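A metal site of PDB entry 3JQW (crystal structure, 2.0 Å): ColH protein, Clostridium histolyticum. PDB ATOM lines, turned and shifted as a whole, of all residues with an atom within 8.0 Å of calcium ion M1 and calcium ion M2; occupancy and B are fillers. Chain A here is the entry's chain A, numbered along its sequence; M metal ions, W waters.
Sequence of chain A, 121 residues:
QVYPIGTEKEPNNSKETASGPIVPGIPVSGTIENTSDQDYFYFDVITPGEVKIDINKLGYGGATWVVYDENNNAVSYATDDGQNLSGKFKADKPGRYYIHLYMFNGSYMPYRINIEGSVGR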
ATOM      1  N   GLU A   8     -30.269  26.813   7.934  1.00  0.00           N
ATOM      2  CA  GLU A   8     -29.349  26.119   7.060  1.00  0.00           C
ATOM      3  C   GLU A   8     -29.961  25.731   5.718  1.00  0.00           C
ATOM      4  O   GLU A   8     -31.178  25.629   5.563  1.00  0.00           O
ATOM      5  CB  GLU A   8     -28.713  24.890   7.749  1.00  0.00           C
ATOM      6  CG  GLU A   8     -29.701  23.779   8.132  1.00  0.00           C
ATOM      7  CD  GLU A   8     -29.015  22.498   8.579  1.00  0.00           C
ATOM      8  OE1 GLU A   8     -27.806  22.295   8.242  1.00  0.00           O
ATOM      9  OE2 GLU A   8     -29.689  21.658   9.223  1.00  0.00           O
ATOM     10  N   LYS A   9     -29.103  25.485   4.735  1.00  0.00           N
ATOM     11  CA  LYS A   9     -29.557  25.028   3.463  1.00  0.00           C
ATOM     12  C   LYS A   9     -28.738  23.845   3.036  1.00  0.00           C
ATOM     13  O   LYS A   9     -27.608  24.006   2.611  1.00  0.00           O
ATOM     14  CB  LYS A   9     -29.473  26.164   2.422  1.00  0.00           C
ATOM     15  CG  LYS A   9     -30.071  25.809   1.085  1.00  0.00           C
ATOM     16  CD  LYS A   9     -30.896  26.996   0.547  1.00  0.00           C
ATOM     17  CE  LYS A   9     -31.427  26.708  -0.862  1.00  0.00           C
ATOM     18  NZ  LYS A   9     -31.805  25.256  -1.030  1.00  0.00           N
ATOM     19  N   GLU A  10     -29.319  22.640   3.147  1.00  0.00           N
ATOM     20  CA  GLU A  10     -28.631  21.412   2.811  1.00  0.00           C
ATOM     21  C   GLU A  10     -28.606  21.301   1.302  1.00  0.00           C
ATOM     22  O   GLU A  10     -29.533  21.804   0.656  1.00  0.00           O
ATOM     23  CB  GLU A  10     -29.284  20.174   3.469  1.00  0.00           C
ATOM     24  CG  GLU A  10     -29.166  20.119   5.004  1.00  0.00           C
ATOM     25  CD  GLU A  10     -27.788  19.673   5.503  1.00  0.00           C
ATOM     26  OE1 GLU A  10     -26.903  19.393   4.675  1.00  0.00           O
ATOM     27  OE2 GLU A  10     -27.583  19.624   6.742  1.00  0.00           O
ATOM     28  N   PRO A  11     -27.522  20.737   0.712  1.00  0.00           N
ATOM     29  CA  PRO A  11     -26.301  20.241   1.416  1.00  0.00           C
ATOM     30  C   PRO A  11     -25.319  21.352   1.774  1.00  0.00           C
ATOM     31  O   PRO A  11     -25.028  22.218   0.963  1.00  0.00           O
ATOM     32  CB  PRO A  11     -25.685  19.283   0.410  1.00  0.00           C
ATOM     33  CG  PRO A  11     -26.141  19.835  -0.977  1.00  0.00           C
ATOM     34  CD  PRO A  11     -27.464  20.543  -0.749  1.00  0.00           C
ATOM     35  N   ASN A  12     -24.820  21.342   2.999  1.00  0.00           N
ATOM     36  CA  ASN A  12     -23.846  22.327   3.444  1.00  0.00           C
ATOM     37  C   ASN A  12     -22.683  21.597   4.171  1.00  0.00           C
ATOM     38  O   ASN A  12     -22.234  22.022   5.203  1.00  0.00           O
ATOM     39  CB  ASN A  12     -24.502  23.348   4.387  1.00  0.00           C
ATOM     40  CG  ASN A  12     -25.108  22.686   5.637  1.00  0.00           C
ATOM     41  OD1 ASN A  12     -25.033  21.469   5.765  1.00  0.00           O
ATOM     42  ND2 ASN A  12     -25.659  23.487   6.544  1.00  0.00           N
ATOM     43  N   ASN A  13     -22.241  20.474   3.600  1.00  0.00           N
ATOM     44  CA  ASN A  13     -21.419  19.498   4.300  1.00  0.00           C
ATOM     45  C   ASN A  13     -19.934  19.712   4.066  1.00  0.00           C
ATOM     46  O   ASN A  13     -19.109  18.907   4.489  1.00  0.00           O
ATOM     47  CB  ASN A  13     -21.789  18.068   3.894  1.00  0.00           C
ATOM     48  CG  ASN A  13     -23.286  17.837   3.906  1.00  0.00           C
ATOM     49  OD1 ASN A  13     -23.965  18.113   4.882  1.00  0.00           O
ATOM     50  ND2 ASN A  13     -23.809  17.287   2.800  1.00  0.00           N
ATOM     51  N   SER A  14     -19.598  20.823   3.406  1.00  0.00           N
ATOM     52  CA  SER A  14     -18.214  21.233   3.236  1.00  0.00           C
ATOM     53  C   SER A  14     -18.135  22.754   3.301  1.00  0.00           C
ATOM     54  O   SER A  14     -19.149  23.476   3.171  1.00  0.00           O
ATOM     55  CB  SER A  14     -17.675  20.745   1.882  1.00  0.00           C
ATOM     56  OG  SER A  14     -18.366  21.426   0.846  1.00  0.00           O
ATOM     57  N   THR A  17     -19.700  24.485   0.409  1.00  0.00           N
ATOM     58  CA  THR A  17     -21.186  24.552   0.377  1.00  0.00           C
ATOM     59  C   THR A  17     -21.805  25.151   1.631  1.00  0.00           C
ATOM     60  O   THR A  17     -22.982  24.934   1.908  1.00  0.00           O
ATOM     61  CB  THR A  17     -21.837  23.175   0.121  1.00  0.00           C
ATOM     62  OG1 THR A  17     -21.242  22.175   0.973  1.00  0.00           O
ATOM     63  CG2 THR A  17     -21.709  22.768  -1.339  1.00  0.00           C
ATOM     64  N   SER A  19     -23.587  27.311   4.450  1.00  0.00           N
ATOM     65  CA  SER A  19     -24.815  28.138   4.422  1.00  0.00           C
ATOM     66  C   SER A  19     -24.478  29.504   4.987  1.00  0.00           C
ATOM     67  O   SER A  19     -23.884  29.573   6.039  1.00  0.00           O
ATOM     68  CB  SER A  19     -25.923  27.537   5.321  1.00  0.00           C
ATOM     69  OG  SER A  19     -26.298  26.231   4.937  1.00  0.00           O
ATOM     70  N   SER A  29     -31.615  28.477  12.320  1.00  0.00           N
ATOM     71  CA  SER A  29     -32.087  27.181  12.796  1.00  0.00           C
ATOM     72  C   SER A  29     -31.463  26.105  11.943  1.00  0.00           C
ATOM     73  O   SER A  29     -31.248  26.313  10.772  1.00  0.00           O
ATOM     74  CB  SER A  29     -33.576  27.087  12.594  1.00  0.00           C
ATOM     75  OG  SER A  29     -34.183  27.875  13.608  1.00  0.00           O
ATOM     76  N   GLY A  30     -31.311  24.919  12.489  1.00  0.00           N
ATOM     77  CA  GLY A  30     -30.971  23.773  11.646  1.00  0.00           C
ATOM     78  C   GLY A  30     -31.040  22.539  12.498  1.00  0.00           C
ATOM     79  O   GLY A  30     -31.503  22.618  13.633  1.00  0.00           O
ATOM     80  N   THR A  31     -30.581  21.425  11.959  1.00  0.00           N
ATOM     81  CA  THR A  31     -30.637  20.138  12.617  1.00  0.00           C
ATOM     82  C   THR A  31     -29.420  19.325  12.191  1.00  0.00           C
ATOM     83  O   THR A  31     -29.091  19.303  10.978  1.00  0.00           O
ATOM     84  CB  THR A  31     -31.950  19.363  12.218  1.00  0.00           C
ATOM     85  OG1 THR A  31     -33.090  20.081  12.729  1.00  0.00           O
ATOM     86  CG2 THR A  31     -31.975  18.019  12.841  1.00  0.00           C
ATOM     87  N   ILE A  32     -28.725  18.726  13.154  1.00  0.00           N
ATOM     88  CA  ILE A  32     -27.734  17.723  12.816  1.00  0.00           C
ATOM     89  C   ILE A  32     -28.497  16.404  12.711  1.00  0.00           C
ATOM     90  O   ILE A  32     -28.941  15.888  13.715  1.00  0.00           O
ATOM     91  CB  ILE A  32     -26.565  17.650  13.807  1.00  0.00           C
ATOM     92  CG1 ILE A  32     -25.998  19.054  14.060  1.00  0.00           C
ATOM     93  CG2 ILE A  32     -25.435  16.738  13.297  1.00  0.00           C
ATOM     94  CD1 ILE A  32     -25.074  19.101  15.329  1.00  0.00           C
ATOM     95  N   GLU A  33     -28.706  15.930  11.472  1.00  0.00           N
ATOM     96  CA  GLU A  33     -29.568  14.758  11.197  1.00  0.00           C
ATOM     97  C   GLU A  33     -29.110  13.485  11.884  1.00  0.00           C
ATOM     98  O   GLU A  33     -29.926  12.660  12.289  1.00  0.00           O
ATOM     99  CB  GLU A  33     -29.702  14.524   9.703  1.00  0.00           C
ATOM    100  CG  GLU A  33     -30.385  15.663   8.996  1.00  0.00           C
ATOM    101  CD  GLU A  33     -31.867  15.772   9.328  1.00  0.00           C
ATOM    102  OE1 GLU A  33     -32.526  14.705   9.566  1.00  0.00           O
ATOM    103  OE2 GLU A  33     -32.400  16.917   9.355  1.00  0.00           O
ATOM    104  N   ASN A  34     -27.790  13.331  12.004  1.00  0.00           N
ATOM    105  CA  ASN A  34     -27.164  12.222  12.678  1.00  0.00           C
ATOM    106  C   ASN A  34     -25.680  12.558  12.649  1.00  0.00           C
ATOM    107  O   ASN A  34     -25.319  13.593  12.101  1.00  0.00           O
ATOM    108  CB  ASN A  34     -27.468  10.882  11.980  1.00  0.00           C
ATOM    109  CG  ASN A  34     -27.234  10.932  10.456  1.00  0.00           C
ATOM    110  OD1 ASN A  34     -26.165  11.285   9.992  1.00  0.00           O
ATOM    111  ND2 ASN A  34     -28.228  10.526   9.684  1.00  0.00           N
ATOM    112  N   SER A  36     -23.235  11.666  10.890  1.00  0.00           N
ATOM    113  CA  SER A  36     -22.659  11.866   9.552  1.00  0.00           C
ATOM    114  C   SER A  36     -22.988  13.217   8.894  1.00  0.00           C
ATOM    115  O   SER A  36     -22.386  13.573   7.876  1.00  0.00           O
ATOM    116  CB  SER A  36     -23.096  10.736   8.614  1.00  0.00           C
ATOM    117  OG  SER A  36     -22.622   9.483   9.079  1.00  0.00           O
ATOM    118  N   ASP A  37     -23.937  13.959   9.462  1.00  0.00           N
ATOM    119  CA  ASP A  37     -24.307  15.243   8.903  1.00  0.00           C
ATOM    120  C   ASP A  37     -23.388  16.346   9.455  1.00  0.00           C
ATOM    121  O   ASP A  37     -23.417  16.668  10.646  1.00  0.00           O
ATOM    122  CB  ASP A  37     -25.742  15.557   9.276  1.00  0.00           C
ATOM    123  CG  ASP A  37     -26.236  16.837   8.626  1.00  0.00           C
ATOM    124  OD1 ASP A  37     -25.769  17.214   7.532  1.00  0.00           O
ATOM    125  OD2 ASP A  37     -27.126  17.463   9.213  1.00  0.00           O
ATOM    126  N   GLN A  38     -22.521  16.865   8.603  1.00  0.00           N
ATOM    127  CA  GLN A  38     -21.671  17.962   8.981  1.00  0.00           C
ATOM    128  C   GLN A  38     -22.408  19.205   8.533  1.00  0.00           C
ATOM    129  O   GLN A  38     -22.925  19.244   7.410  1.00  0.00           O
ATOM    130  CB  GLN A  38     -20.311  17.863   8.238  1.00  0.00           C
ATOM    131  CG  GLN A  38     -19.578  16.487   8.399  1.00  0.00           C
ATOM    132  CD  GLN A  38     -18.937  16.359   9.746  1.00  0.00           C
ATOM    133  OE1 GLN A  38     -18.428  17.336  10.269  1.00  0.00           O
ATOM    134  NE2 GLN A  38     -18.936  15.164  10.290  1.00  0.00           N
ATOM    135  N   ASP A  39     -22.417  20.243   9.361  1.00  0.00           N
ATOM    136  CA  ASP A  39     -23.073  21.493   8.979  1.00  0.00           C
ATOM    137  C   ASP A  39     -22.064  22.663   8.980  1.00  0.00           C
ATOM    138  O   ASP A  39     -21.573  23.056  10.027  1.00  0.00           O
ATOM    139  CB  ASP A  39     -24.249  21.811   9.895  1.00  0.00           C
ATOM    140  CG  ASP A  39     -25.449  20.862   9.700  1.00  0.00           C
ATOM    141  OD1 ASP A  39     -25.461  20.044   8.761  1.00  0.00           O
ATOM    142  OD2 ASP A  39     -26.400  20.942  10.464  1.00  0.00           O
ATOM    143  N   TYR A  40     -21.806  23.232   7.800  1.00  0.00           N
ATOM    144  CA  TYR A  40     -20.932  24.380   7.706  1.00  0.00           C
ATOM    145  C   TYR A  40     -21.731  25.633   7.372  1.00  0.00           C
ATOM    146  O   TYR A  40     -22.683  25.590   6.533  1.00  0.00           O
ATOM    147  CB  TYR A  40     -19.855  24.181   6.611  1.00  0.00           C
ATOM    148  CG  TYR A  40     -18.803  23.125   6.872  1.00  0.00           C
ATOM    149  CD1 TYR A  40     -17.490  23.481   7.194  1.00  0.00           C
ATOM    150  CD2 TYR A  40     -19.112  21.778   6.733  1.00  0.00           C
ATOM    151  CE1 TYR A  40     -16.509  22.494   7.421  1.00  0.00           C
ATOM    152  CE2 TYR A  40     -18.174  20.803   6.924  1.00  0.00           C
ATOM    153  CZ  TYR A  40     -16.869  21.146   7.255  1.00  0.00           C
ATOM    154  OH  TYR A  40     -15.968  20.123   7.430  1.00  0.00           O
ATOM    155  N   PHE A  41     -21.299  26.733   8.013  1.00  0.00           N
ATOM    156  CA  PHE A  41     -21.932  28.070   7.865  1.00  0.00           C
ATOM    157  C   PHE A  41     -20.848  29.085   7.635  1.00  0.00           C
ATOM    158  O   PHE A  41     -19.688  28.816   7.953  1.00  0.00           O
ATOM    159  CB  PHE A  41     -22.688  28.469   9.119  1.00  0.00           C
ATOM    160  CG  PHE A  41     -23.829  27.550   9.434  1.00  0.00           C
ATOM    161  CD1 PHE A  41     -25.118  27.815   8.931  1.00  0.00           C
ATOM    162  CD2 PHE A  41     -23.623  26.394  10.178  1.00  0.00           C
ATOM    163  CE1 PHE A  41     -26.182  26.959   9.214  1.00  0.00           C
ATOM    164  CE2 PHE A  41     -24.663  25.532  10.475  1.00  0.00           C
ATOM    165  CZ  PHE A  41     -25.946  25.816   9.985  1.00  0.00           C
ATOM    166  N   LEU A 101     -19.823  22.928  12.326  1.00  0.00           N
ATOM    167  CA  LEU A 101     -20.641  22.338  13.396  1.00  0.00           C
ATOM    168  C   LEU A 101     -20.867  20.837  13.144  1.00  0.00           C
ATOM    169  O   LEU A 101     -21.223  20.451  12.057  1.00  0.00           O
ATOM    170  CB  LEU A 101     -22.002  23.067  13.509  1.00  0.00           C
ATOM    171  CG  LEU A 101     -23.072  22.563  14.490  1.00  0.00           C
ATOM    172  CD1 LEU A 101     -22.626  22.630  15.930  1.00  0.00           C
ATOM    173  CD2 LEU A 101     -24.495  23.281  14.341  1.00  0.00           C
ATOM    174  N   MET A 109     -30.092  16.228  16.406  1.00  0.00           N
ATOM    175  CA  MET A 109     -29.989  17.422  17.213  1.00  0.00           C
ATOM    176  C   MET A 109     -30.388  18.696  16.511  1.00  0.00           C
ATOM    177  O   MET A 109     -29.574  19.258  15.786  1.00  0.00           O
ATOM    178  CB  MET A 109     -28.547  17.607  17.758  1.00  0.00           C
ATOM    179  CG  MET A 109     -28.549  18.636  18.934  1.00  0.00           C
ATOM    180  SD  MET A 109     -26.885  18.954  19.372  1.00  0.00           S
ATOM    181  CE  MET A 109     -26.499  17.533  20.365  1.00  0.00           C
ATOM    182  N   TYR A 111     -30.857  22.682  16.476  1.00  0.00           N
ATOM    183  CA  TYR A 111     -30.022  23.705  17.151  1.00  0.00           C
ATOM    184  C   TYR A 111     -30.428  25.096  16.676  1.00  0.00           C
ATOM    185  O   TYR A 111     -31.210  25.250  15.718  1.00  0.00           O
ATOM    186  CB  TYR A 111     -28.498  23.474  16.910  1.00  0.00           C
ATOM    187  CG  TYR A 111     -28.149  23.458  15.432  1.00  0.00           C
ATOM    188  CD1 TYR A 111     -28.025  24.644  14.695  1.00  0.00           C
ATOM    189  CD2 TYR A 111     -28.033  22.271  14.757  1.00  0.00           C
ATOM    190  CE1 TYR A 111     -27.732  24.616  13.325  1.00  0.00           C
ATOM    191  CE2 TYR A 111     -27.728  22.210  13.408  1.00  0.00           C
ATOM    192  CZ  TYR A 111     -27.592  23.378  12.701  1.00  0.00           C
ATOM    193  OH  TYR A 111     -27.316  23.278  11.386  1.00  0.00           O
HETATM  194 CA    CA M   1     -27.994  19.785   8.950  1.00  0.00          CA
HETATM  195 CA    CA M   2     -25.139  19.256   6.583  1.00  0.00          CA
HETATM  196  O   HOH W   1     -30.063  18.715   8.289  1.00  0.00           O
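OD2 of Asp 39 lies close to OH of Tyr 111 (2.7 Å). The side-chain hydroxyl of Ser 19 is in hydrogen-bond range of the side-chain amide nitrogen of Asn 12 (3.2 Å). OD2 of Asp 37 lies close to N of Glu 33, at 3.2 Å. The side-chain carboxylate of Glu 8 lies close to the side-chain hydroxyl of Tyr 111 (3.3 Å). The backbone carbonyl oxygen (O) of Asn 12 is in hydrogen-bond range of the backbone NH (N) of Tyr 40 (2.9 Å). O of Asp 39 is in hydrogen-bond range of N of Leu 101 (2.9 Å). N of Glu 8 lies within hydrogen-bond range of O of Ser 29 (3.0 Å). The side-chain carboxylate of Glu 8 lies close to the side-chain amide nitrogen of Asn 12, 3.0 Å away.
Five residues have an atom within 4 Å of calcium ion M1: Glu 8, Glu 10, Thr 31, Asp 37 and Asp 39. The nearest printed residue that does not touch calcium ion M1 is Tyr 111 (4.3 Å).
Six residues have an atom within 4 Å of calcium ion M2: Glu 10, Asn 12, Asn 13, Asp 37, Gln 38 and Asp 39.
Calcium ion M1 is bound by the side-chain carboxylate (OE2) of Glu 10, the backbone carbonyl oxygen (O) of Thr 31, water W1, the side-chain carboxylate (OD2) of Asp 39, the side-chain carboxylate (OD2) of Asp 37, the side-chain carboxylate (OE2) of Glu 8, the side-chain carboxylate (OD1) of Asp 39 and the side-chain carboxylate (OE1) of Glu 8.
Calcium ion M2 is bound by OD1 of Asp 37 (2.3 Å), OD1 of Asp 39 (2.3 Å), OD1 of Asn 12 (2.4 Å), OD1 of Asn 13 (2.4 Å), O of Gln 38 (2.4 Å), OE2 of Glu 10 (2.5 Å) and OE1 of Glu 10 (2.6 Å). Calcium ion M2 has seven donor atoms within binding distance.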
